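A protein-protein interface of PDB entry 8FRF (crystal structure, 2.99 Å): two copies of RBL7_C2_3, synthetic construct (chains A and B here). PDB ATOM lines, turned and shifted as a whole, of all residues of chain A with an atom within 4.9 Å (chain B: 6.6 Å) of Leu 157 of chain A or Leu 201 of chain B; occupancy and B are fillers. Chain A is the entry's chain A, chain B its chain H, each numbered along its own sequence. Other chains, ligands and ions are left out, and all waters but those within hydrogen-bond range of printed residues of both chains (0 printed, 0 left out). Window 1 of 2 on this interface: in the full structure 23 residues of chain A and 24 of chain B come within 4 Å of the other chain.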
ATOM      1  N   MET A 153      15.125 -32.785  26.725  1.00  0.00           N
ATOM      2  CA  MET A 153      16.523 -33.147  26.937  1.00  0.00           C
ATOM      3  C   MET A 153      17.380 -31.920  27.214  1.00  0.00           C
ATOM      4  O   MET A 153      18.149 -31.896  28.182  1.00  0.00           O
ATOM      5  CB  MET A 153      17.055 -33.909  25.727  1.00  0.00           C
ATOM      6  CG  MET A 153      18.487 -34.398  25.887  1.00  0.00           C
ATOM      7  SD  MET A 153      18.700 -35.717  27.089  1.00  0.00           S
ATOM      8  CE  MET A 153      20.449 -36.052  26.881  1.00  0.00           C
ATOM      9  N   SER A 154      17.258 -30.882  26.380  1.00  0.00           N
ATOM     10  CA  SER A 154      18.080 -29.695  26.591  1.00  0.00           C
ATOM     11  C   SER A 154      17.670 -28.969  27.867  1.00  0.00           C
ATOM     12  O   SER A 154      18.523 -28.412  28.568  1.00  0.00           O
ATOM     13  CB  SER A 154      18.014 -28.760  25.377  1.00  0.00           C
ATOM     14  OG  SER A 154      16.721 -28.219  25.182  1.00  0.00           O
ATOM     15  N   LEU A 155      16.372 -28.957  28.185  1.00  0.00           N
ATOM     16  CA  LEU A 155      15.939 -28.360  29.444  1.00  0.00           C
ATOM     17  C   LEU A 155      16.482 -29.136  30.633  1.00  0.00           C
ATOM     18  O   LEU A 155      16.754 -28.552  31.689  1.00  0.00           O
ATOM     19  CB  LEU A 155      14.415 -28.289  29.510  1.00  0.00           C
ATOM     20  CG  LEU A 155      13.772 -27.305  28.536  1.00  0.00           C
ATOM     21  CD1 LEU A 155      12.271 -27.317  28.694  1.00  0.00           C
ATOM     22  CD2 LEU A 155      14.322 -25.915  28.767  1.00  0.00           C
ATOM     23  N   LEU A 156      16.649 -30.450  30.482  1.00  0.00           N
ATOM     24  CA  LEU A 156      17.244 -31.234  31.554  1.00  0.00           C
ATOM     25  C   LEU A 156      18.698 -30.834  31.765  1.00  0.00           C
ATOM     26  O   LEU A 156      19.141 -30.645  32.904  1.00  0.00           O
ATOM     27  CB  LEU A 156      17.128 -32.724  31.227  1.00  0.00           C
ATOM     28  CG  LEU A 156      17.187 -33.705  32.400  1.00  0.00           C
ATOM     29  CD1 LEU A 156      16.260 -34.860  32.122  1.00  0.00           C
ATOM     30  CD2 LEU A 156      18.599 -34.206  32.650  1.00  0.00           C
ATOM     31  N   LEU A 157      19.445 -30.668  30.672  1.00  0.00           N
ATOM     32  CA  LEU A 157      20.822 -30.204  30.786  1.00  0.00           C
ATOM     33  C   LEU A 157      20.877 -28.773  31.308  1.00  0.00           C
ATOM     34  O   LEU A 157      21.760 -28.429  32.104  1.00  0.00           O
ATOM     35  CB  LEU A 157      21.518 -30.297  29.428  1.00  0.00           C
ATOM     36  CG  LEU A 157      21.308 -31.575  28.620  1.00  0.00           C
ATOM     37  CD1 LEU A 157      21.883 -31.417  27.215  1.00  0.00           C
ATOM     38  CD2 LEU A 157      21.925 -32.764  29.340  1.00  0.00           C
ATOM     39  N   LEU A 158      19.933 -27.930  30.882  1.00  0.00           N
ATOM     40  CA  LEU A 158      19.875 -26.566  31.390  1.00  0.00           C
ATOM     41  C   LEU A 158      19.628 -26.565  32.891  1.00  0.00           C
ATOM     42  O   LEU A 158      20.162 -25.717  33.616  1.00  0.00           O
ATOM     43  CB  LEU A 158      18.782 -25.784  30.660  1.00  0.00           C
ATOM     44  CG  LEU A 158      18.737 -24.260  30.789  1.00  0.00           C
ATOM     45  CD1 LEU A 158      19.984 -23.623  30.180  1.00  0.00           C
ATOM     46  CD2 LEU A 158      17.465 -23.699  30.153  1.00  0.00           C
ATOM     47  N   LEU A 159      18.821 -27.517  33.376  1.00  0.00           N
ATOM     48  CA  LEU A 159      18.569 -27.622  34.810  1.00  0.00           C
ATOM     49  C   LEU A 159      19.779 -28.177  35.545  1.00  0.00           C
ATOM     50  O   LEU A 159      20.107 -27.715  36.643  1.00  0.00           O
ATOM     51  CB  LEU A 159      17.339 -28.487  35.070  1.00  0.00           C
ATOM     52  CG  LEU A 159      16.003 -27.766  34.893  1.00  0.00           C
ATOM     53  CD1 LEU A 159      14.848 -28.700  35.164  1.00  0.00           C
ATOM     54  CD2 LEU A 159      15.942 -26.578  35.820  1.00  0.00           C
ATOM     55  N   LEU A 160      20.455 -29.169  34.959  1.00  0.00           N
ATOM     56  CA  LEU A 160      21.669 -29.691  35.578  1.00  0.00           C
ATOM     57  C   LEU A 160      22.734 -28.611  35.687  1.00  0.00           C
ATOM     58  O   LEU A 160      23.435 -28.521  36.702  1.00  0.00           O
ATOM     59  CB  LEU A 160      22.203 -30.883  34.784  1.00  0.00           C
ATOM     60  CG  LEU A 160      21.383 -32.168  34.844  1.00  0.00           C
ATOM     61  CD1 LEU A 160      21.910 -33.178  33.844  1.00  0.00           C
ATOM     62  CD2 LEU A 160      21.420 -32.741  36.257  1.00  0.00           C
ATOM     63  N   LEU A 161      22.869 -27.780  34.652  1.00  0.00           N
ATOM     64  CA  LEU A 161      23.793 -26.655  34.726  1.00  0.00           C
ATOM     65  C   LEU A 161      23.403 -25.693  35.839  1.00  0.00           C
ATOM     66  O   LEU A 161      24.274 -25.077  36.464  1.00  0.00           O
ATOM     67  CB  LEU A 161      23.843 -25.934  33.380  1.00  0.00           C
ATOM     68  CG  LEU A 161      24.522 -26.691  32.232  1.00  0.00           C
ATOM     69  CD1 LEU A 161      24.165 -26.060  30.901  1.00  0.00           C
ATOM     70  CD2 LEU A 161      26.032 -26.764  32.400  1.00  0.00           C
ATOM     71  N   LEU A 198      22.465 -39.872  29.164  1.00  0.00           N
ATOM     72  CA  LEU A 198      22.259 -39.445  30.541  1.00  0.00           C
ATOM     73  C   LEU A 198      22.761 -40.492  31.522  1.00  0.00           C
ATOM     74  O   LEU A 198      23.269 -40.147  32.596  1.00  0.00           O
ATOM     75  CB  LEU A 198      20.778 -39.142  30.776  1.00  0.00           C
ATOM     76  CG  LEU A 198      20.263 -37.908  30.027  1.00  0.00           C
ATOM     77  CD1 LEU A 198      18.757 -37.733  30.195  1.00  0.00           C
ATOM     78  CD2 LEU A 198      21.013 -36.660  30.478  1.00  0.00           C
ATOM     79  N   MET B 153      29.029 -37.352  23.530  1.00  0.00           N
ATOM     80  CA  MET B 153      27.919 -36.535  24.011  1.00  0.00           C
ATOM     81  C   MET B 153      27.963 -36.372  25.525  1.00  0.00           C
ATOM     82  O   MET B 153      27.863 -35.253  26.041  1.00  0.00           O
ATOM     83  CB  MET B 153      26.588 -37.150  23.579  1.00  0.00           C
ATOM     84  CG  MET B 153      25.383 -36.316  23.967  1.00  0.00           C
ATOM     85  SD  MET B 153      25.273 -34.770  23.060  1.00  0.00           S
ATOM     86  CE  MET B 153      23.724 -34.126  23.695  1.00  0.00           C
ATOM     87  N   LEU B 157      28.794 -32.888  28.020  1.00  0.00           N
ATOM     88  CA  LEU B 157      28.022 -32.390  29.151  1.00  0.00           C
ATOM     89  C   LEU B 157      28.862 -32.403  30.414  1.00  0.00           C
ATOM     90  O   LEU B 157      28.748 -31.501  31.256  1.00  0.00           O
ATOM     91  CB  LEU B 157      26.761 -33.230  29.345  1.00  0.00           C
ATOM     92  CG  LEU B 157      25.954 -33.532  28.086  1.00  0.00           C
ATOM     93  CD1 LEU B 157      24.862 -34.547  28.384  1.00  0.00           C
ATOM     94  CD2 LEU B 157      25.364 -32.236  27.543  1.00  0.00           C
ATOM     95  N   LEU B 160      30.908 -29.306  30.112  1.00  0.00           N
ATOM     96  CA  LEU B 160      30.108 -28.111  30.353  1.00  0.00           C
ATOM     97  C   LEU B 160      29.838 -27.917  31.840  1.00  0.00           C
ATOM     98  O   LEU B 160      29.931 -26.794  32.354  1.00  0.00           O
ATOM     99  CB  LEU B 160      28.789 -28.202  29.586  1.00  0.00           C
ATOM    100  CG  LEU B 160      28.838 -28.118  28.066  1.00  0.00           C
ATOM    101  CD1 LEU B 160      27.466 -28.423  27.480  1.00  0.00           C
ATOM    102  CD2 LEU B 160      29.331 -26.750  27.621  1.00  0.00           C
ATOM    103  N   LEU B 161      29.510 -29.002  32.548  1.00  0.00           N
ATOM    104  CA  LEU B 161      29.361 -28.934  33.997  1.00  0.00           C
ATOM    105  C   LEU B 161      30.669 -28.555  34.680  1.00  0.00           C
ATOM    106  O   LEU B 161      30.654 -27.906  35.732  1.00  0.00           O
ATOM    107  CB  LEU B 161      28.847 -30.271  34.528  1.00  0.00           C
ATOM    108  CG  LEU B 161      27.392 -30.595  34.182  1.00  0.00           C
ATOM    109  CD1 LEU B 161      27.095 -32.073  34.394  1.00  0.00           C
ATOM    110  CD2 LEU B 161      26.449 -29.738  35.004  1.00  0.00           C
ATOM    111  N   GLU B 196      20.334 -31.129  17.676  1.00  0.00           N
ATOM    112  CA  GLU B 196      19.194 -30.296  18.050  1.00  0.00           C
ATOM    113  C   GLU B 196      19.137 -30.075  19.556  1.00  0.00           C
ATOM    114  O   GLU B 196      18.775 -28.985  20.015  1.00  0.00           O
ATOM    115  CB  GLU B 196      17.893 -30.922  17.548  1.00  0.00           C
ATOM    116  CG  GLU B 196      17.740 -30.877  16.028  1.00  0.00           C
ATOM    117  CD  GLU B 196      16.496 -31.600  15.535  1.00  0.00           C
ATOM    118  OE1 GLU B 196      15.581 -31.840  16.354  1.00  0.00           O
ATOM    119  OE2 GLU B 196      16.433 -31.924  14.329  1.00  0.00           O
ATOM    120  N   VAL B 197      19.522 -31.083  20.343  1.00  0.00           N
ATOM    121  CA  VAL B 197      19.565 -30.918  21.792  1.00  0.00           C
ATOM    122  C   VAL B 197      20.586 -29.857  22.178  1.00  0.00           C
ATOM    123  O   VAL B 197      20.286 -28.917  22.924  1.00  0.00           O
ATOM    124  CB  VAL B 197      19.879 -32.259  22.473  1.00  0.00           C
ATOM    125  CG1 VAL B 197      20.290 -32.029  23.919  1.00  0.00           C
ATOM    126  CG2 VAL B 197      18.675 -33.173  22.402  1.00  0.00           C
ATOM    127  N   LEU B 198      21.812 -29.995  21.675  1.00  0.00           N
ATOM    128  CA  LEU B 198      22.863 -29.040  22.008  1.00  0.00           C
ATOM    129  C   LEU B 198      22.573 -27.658  21.439  1.00  0.00           C
ATOM    130  O   LEU B 198      22.919 -26.646  22.062  1.00  0.00           O
ATOM    131  CB  LEU B 198      24.213 -29.559  21.516  1.00  0.00           C
ATOM    132  CG  LEU B 198      24.711 -30.787  22.284  1.00  0.00           C
ATOM    133  CD1 LEU B 198      25.996 -31.335  21.675  1.00  0.00           C
ATOM    134  CD2 LEU B 198      24.903 -30.447  23.758  1.00  0.00           C
ATOM    135  N   LEU B 199      21.946 -27.589  20.265  1.00  0.00           N
ATOM    136  CA  LEU B 199      21.578 -26.291  19.716  1.00  0.00           C
ATOM    137  C   LEU B 199      20.539 -25.586  20.586  1.00  0.00           C
ATOM    138  O   LEU B 199      20.629 -24.371  20.802  1.00  0.00           O
ATOM    139  CB  LEU B 199      21.080 -26.455  18.281  1.00  0.00           C
ATOM    140  CG  LEU B 199      22.177 -26.626  17.221  1.00  0.00           C
ATOM    141  CD1 LEU B 199      21.594 -27.082  15.897  1.00  0.00           C
ATOM    142  CD2 LEU B 199      22.952 -25.326  17.029  1.00  0.00           C
ATOM    143  N   GLN B 200      19.553 -26.323  21.100  1.00  0.00           N
ATOM    144  CA  GLN B 200      18.562 -25.703  21.975  1.00  0.00           C
ATOM    145  C   GLN B 200      19.182 -25.275  23.299  1.00  0.00           C
ATOM    146  O   GLN B 200      18.826 -24.223  23.846  1.00  0.00           O
ATOM    147  CB  GLN B 200      17.401 -26.655  22.222  1.00  0.00           C
ATOM    148  CG  GLN B 200      16.541 -26.900  21.012  1.00  0.00           C
ATOM    149  CD  GLN B 200      15.262 -27.617  21.370  1.00  0.00           C
ATOM    150  OE1 GLN B 200      14.395 -27.060  22.044  1.00  0.00           O
ATOM    151  NE2 GLN B 200      15.140 -28.865  20.931  1.00  0.00           N
ATOM    152  N   LEU B 201      20.085 -26.093  23.845  1.00  0.00           N
ATOM    153  CA  LEU B 201      20.755 -25.721  25.085  1.00  0.00           C
ATOM    154  C   LEU B 201      21.571 -24.449  24.899  1.00  0.00           C
ATOM    155  O   LEU B 201      21.543 -23.551  25.751  1.00  0.00           O
ATOM    156  CB  LEU B 201      21.641 -26.867  25.571  1.00  0.00           C
ATOM    157  CG  LEU B 201      22.419 -26.582  26.858  1.00  0.00           C
ATOM    158  CD1 LEU B 201      21.461 -26.266  28.001  1.00  0.00           C
ATOM    159  CD2 LEU B 201      23.323 -27.753  27.222  1.00  0.00           C
ATOM    160  N   LEU B 202      22.311 -24.357  23.789  1.00  0.00           N
ATOM    161  CA  LEU B 202      23.085 -23.152  23.510  1.00  0.00           C
ATOM    162  C   LEU B 202      22.184 -21.943  23.277  1.00  0.00           C
ATOM    163  O   LEU B 202      22.464 -20.852  23.785  1.00  0.00           O
ATOM    164  CB  LEU B 202      23.996 -23.370  22.301  1.00  0.00           C
ATOM    165  CG  LEU B 202      25.441 -23.805  22.551  1.00  0.00           C
ATOM    166  CD1 LEU B 202      25.498 -25.100  23.352  1.00  0.00           C
ATOM    167  CD2 LEU B 202      26.200 -23.940  21.234  1.00  0.00           C
ATOM    168  N   GLU B 203      21.097 -22.112  22.517  1.00  0.00           N
ATOM    169  CA  GLU B 203      20.249 -20.971  22.182  1.00  0.00           C
ATOM    170  C   GLU B 203      19.581 -20.364  23.409  1.00  0.00           C
ATOM    171  O   GLU B 203      19.137 -19.210  23.355  1.00  0.00           O
ATOM    172  CB  GLU B 203      19.190 -21.351  21.144  1.00  0.00           C
ATOM    173  CG  GLU B 203      18.453 -20.131  20.578  1.00  0.00           C
ATOM    174  CD  GLU B 203      17.321 -20.484  19.636  1.00  0.00           C
ATOM    175  OE1 GLU B 203      16.815 -21.625  19.700  1.00  0.00           O
ATOM    176  OE2 GLU B 203      16.927 -19.607  18.835  1.00  0.00           O
ATOM    177  N   ALA B 204      19.521 -21.090  24.523  1.00  0.00           N
ATOM    178  CA  ALA B 204      18.839 -20.574  25.698  1.00  0.00           C
ATOM    179  C   ALA B 204      19.799 -20.049  26.754  1.00  0.00           C
ATOM    180  O   ALA B 204      19.356 -19.377  27.688  1.00  0.00           O
ATOM    181  CB  ALA B 204      17.949 -21.663  26.314  1.00  0.00           C
ATOM    182  N   ALA B 205      21.101 -20.295  26.606  1.00  0.00           N
ATOM    183  CA  ALA B 205      22.091 -19.721  27.507  1.00  0.00           C
ATOM    184  C   ALA B 205      23.345 -19.283  26.751  1.00  0.00           C
ATOM    185  O   ALA B 205      24.436 -19.239  27.327  1.00  0.00           O
ATOM    186  CB  ALA B 205      22.455 -20.705  28.622  1.00  0.00           C
ATOM    187  N   GLY B 206      23.214 -18.960  25.465  1.00  0.00           N
ATOM    188  CA  GLY B 206      24.356 -18.538  24.675  1.00  0.00           C
ATOM    189  C   GLY B 206      24.735 -17.087  24.898  1.00  0.00           C
ATOM    190  O   GLY B 206      25.914 -16.765  25.085  1.00  0.00           O
ATOM    191  N   TRP B 209      26.088 -17.367  29.277  1.00  0.00           N
ATOM    192  CA  TRP B 209      26.385 -18.703  29.783  1.00  0.00           C
ATOM    193  C   TRP B 209      26.857 -18.579  31.226  1.00  0.00           C
ATOM    194  O   TRP B 209      27.930 -18.025  31.493  1.00  0.00           O
ATOM    195  CB  TRP B 209      27.429 -19.405  28.920  1.00  0.00           C
ATOM    196  CG  TRP B 209      27.567 -20.869  29.243  1.00  0.00           C
ATOM    197  CD1 TRP B 209      28.488 -21.445  30.071  1.00  0.00           C
ATOM    198  CD2 TRP B 209      26.744 -21.940  28.754  1.00  0.00           C
ATOM    199  NE1 TRP B 209      28.296 -22.807  30.120  1.00  0.00           N
ATOM    200  CE2 TRP B 209      27.232 -23.135  29.322  1.00  0.00           C
ATOM    201  CE3 TRP B 209      25.648 -22.003  27.888  1.00  0.00           C
ATOM    202  CZ2 TRP B 209      26.660 -24.373  29.051  1.00  0.00           C
ATOM    203  CZ3 TRP B 209      25.082 -23.235  27.623  1.00  0.00           C
ATOM    204  CH2 TRP B 209      25.589 -24.402  28.200  1.00  0.00           C
ATOM    205  N   HIS B 212      22.462 -18.597  35.153  1.00  0.00           N
ATOM    206  CA  HIS B 212      21.617 -19.397  36.029  1.00  0.00           C
ATOM    207  C   HIS B 212      22.410 -20.442  36.804  1.00  0.00           C
ATOM    208  O   HIS B 212      21.808 -21.328  37.422  1.00  0.00           O
ATOM    209  CB  HIS B 212      20.496 -20.070  35.225  1.00  0.00           C
ATOM    210  CG  HIS B 212      20.980 -21.079  34.230  1.00  0.00           C
ATOM    211  ND1 HIS B 212      21.815 -20.756  33.182  1.00  0.00           N
ATOM    212  CD2 HIS B 212      20.730 -22.406  34.116  1.00  0.00           C
ATOM    213  CE1 HIS B 212      22.065 -21.840  32.470  1.00  0.00           C
ATOM    214  NE2 HIS B 212      21.418 -22.855  33.015  1.00  0.00           N
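Of the printed residues of chain B, Met 153 of chain A touches Val 197.
Leu 157 of chain A touches three residues of chain B.
Of the printed residues of chain A, Val 197 of chain B touches Met 153 (3.6 Å), Ser 154 (3.3 Å) and Leu 157 (3.7 Å).
Leu 198 of chain B touches none of the printed residues of chain A.
Of the printed residues of chain A, Leu 201 of chain B touches Ser 154, Leu 157, Leu 158 and Leu 161.
The nearest residue of chain B that does not touch Leu 157 of chain A is Leu 198 of chain B (4.7 Å).
The nearest printed residue of chain A that does not touch Leu 161 of chain B is Leu 157 of chain A (5.7 Å).
Printed residues of chain A that touch a printed residue of chain B: Met 153, Ser 154, Leu 157, Leu 158, Leu 160 and Leu 161.
Hydrophobic or aromatic side chains of chain A that line the printed part of chain B: Met 153, Leu 157, Leu 158 and Leu 161.
Printed residues of chain B that touch a printed residue of chain A: Leu 157, Leu 160, Leu 161, Val 197, Gln 200, Leu 201, Trp 209 and His 212.
Hydrophobic or aromatic side chains of chain B within 4 Å of the printed part of chain A: Leu 157, Leu 161, Val 197, Leu 201, Trp 209 and His 212.
Among the printed residues, 15 pairs touch across the chains.
Leu 157 of chain B touches its own counterpart, Leu 157 of chain A.
Leu 160 of chain A touches Leu 161 of chain B, and with the chains exchanged Leu 161 of chain A touches Leu 160 of chain B.
Leu 161 of chain A touches its own counterpart, Leu 161 of chain B.
Positions printed for both chains: 153, 157, 160, 161 and 198.
The backbone carbonyl oxygen (O) of Leu 158 of chain A sits at hydrogen-bond distance from a ring nitrogen (NE2) of His 212 of chain B (3.2 Å).
Met 153 of chain A touches Val 197 of chain B (CG to CG1, 3.6 Å).
Ser 154 of chain A touches Val 197 of chain B (CB to O, 3.3 Å).
OG of Ser 154 of chain A touches CB of Gln 200 of chain B, 3.4 Å away.
Ser 154 of chain A touches Leu 201 of chain B (O to CD1, 3.7 Å).
Leu 157 of chain A touches Leu 157 of chain B.
CB of Leu 157 of chain A touches CD2 of Leu 201 of chain B, at 3.8 Å.
CD1 of Leu 201 of chain B touches N of Leu 158 of chain A (3.7 Å).
Leu 160 of chain A touches Leu 161 of chain B (O to CD2, 3.7 Å).
Leu 201 of chain B touches Leu 161 of chain A.
Leu 161 of chain A touches Trp 209 of chain B.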
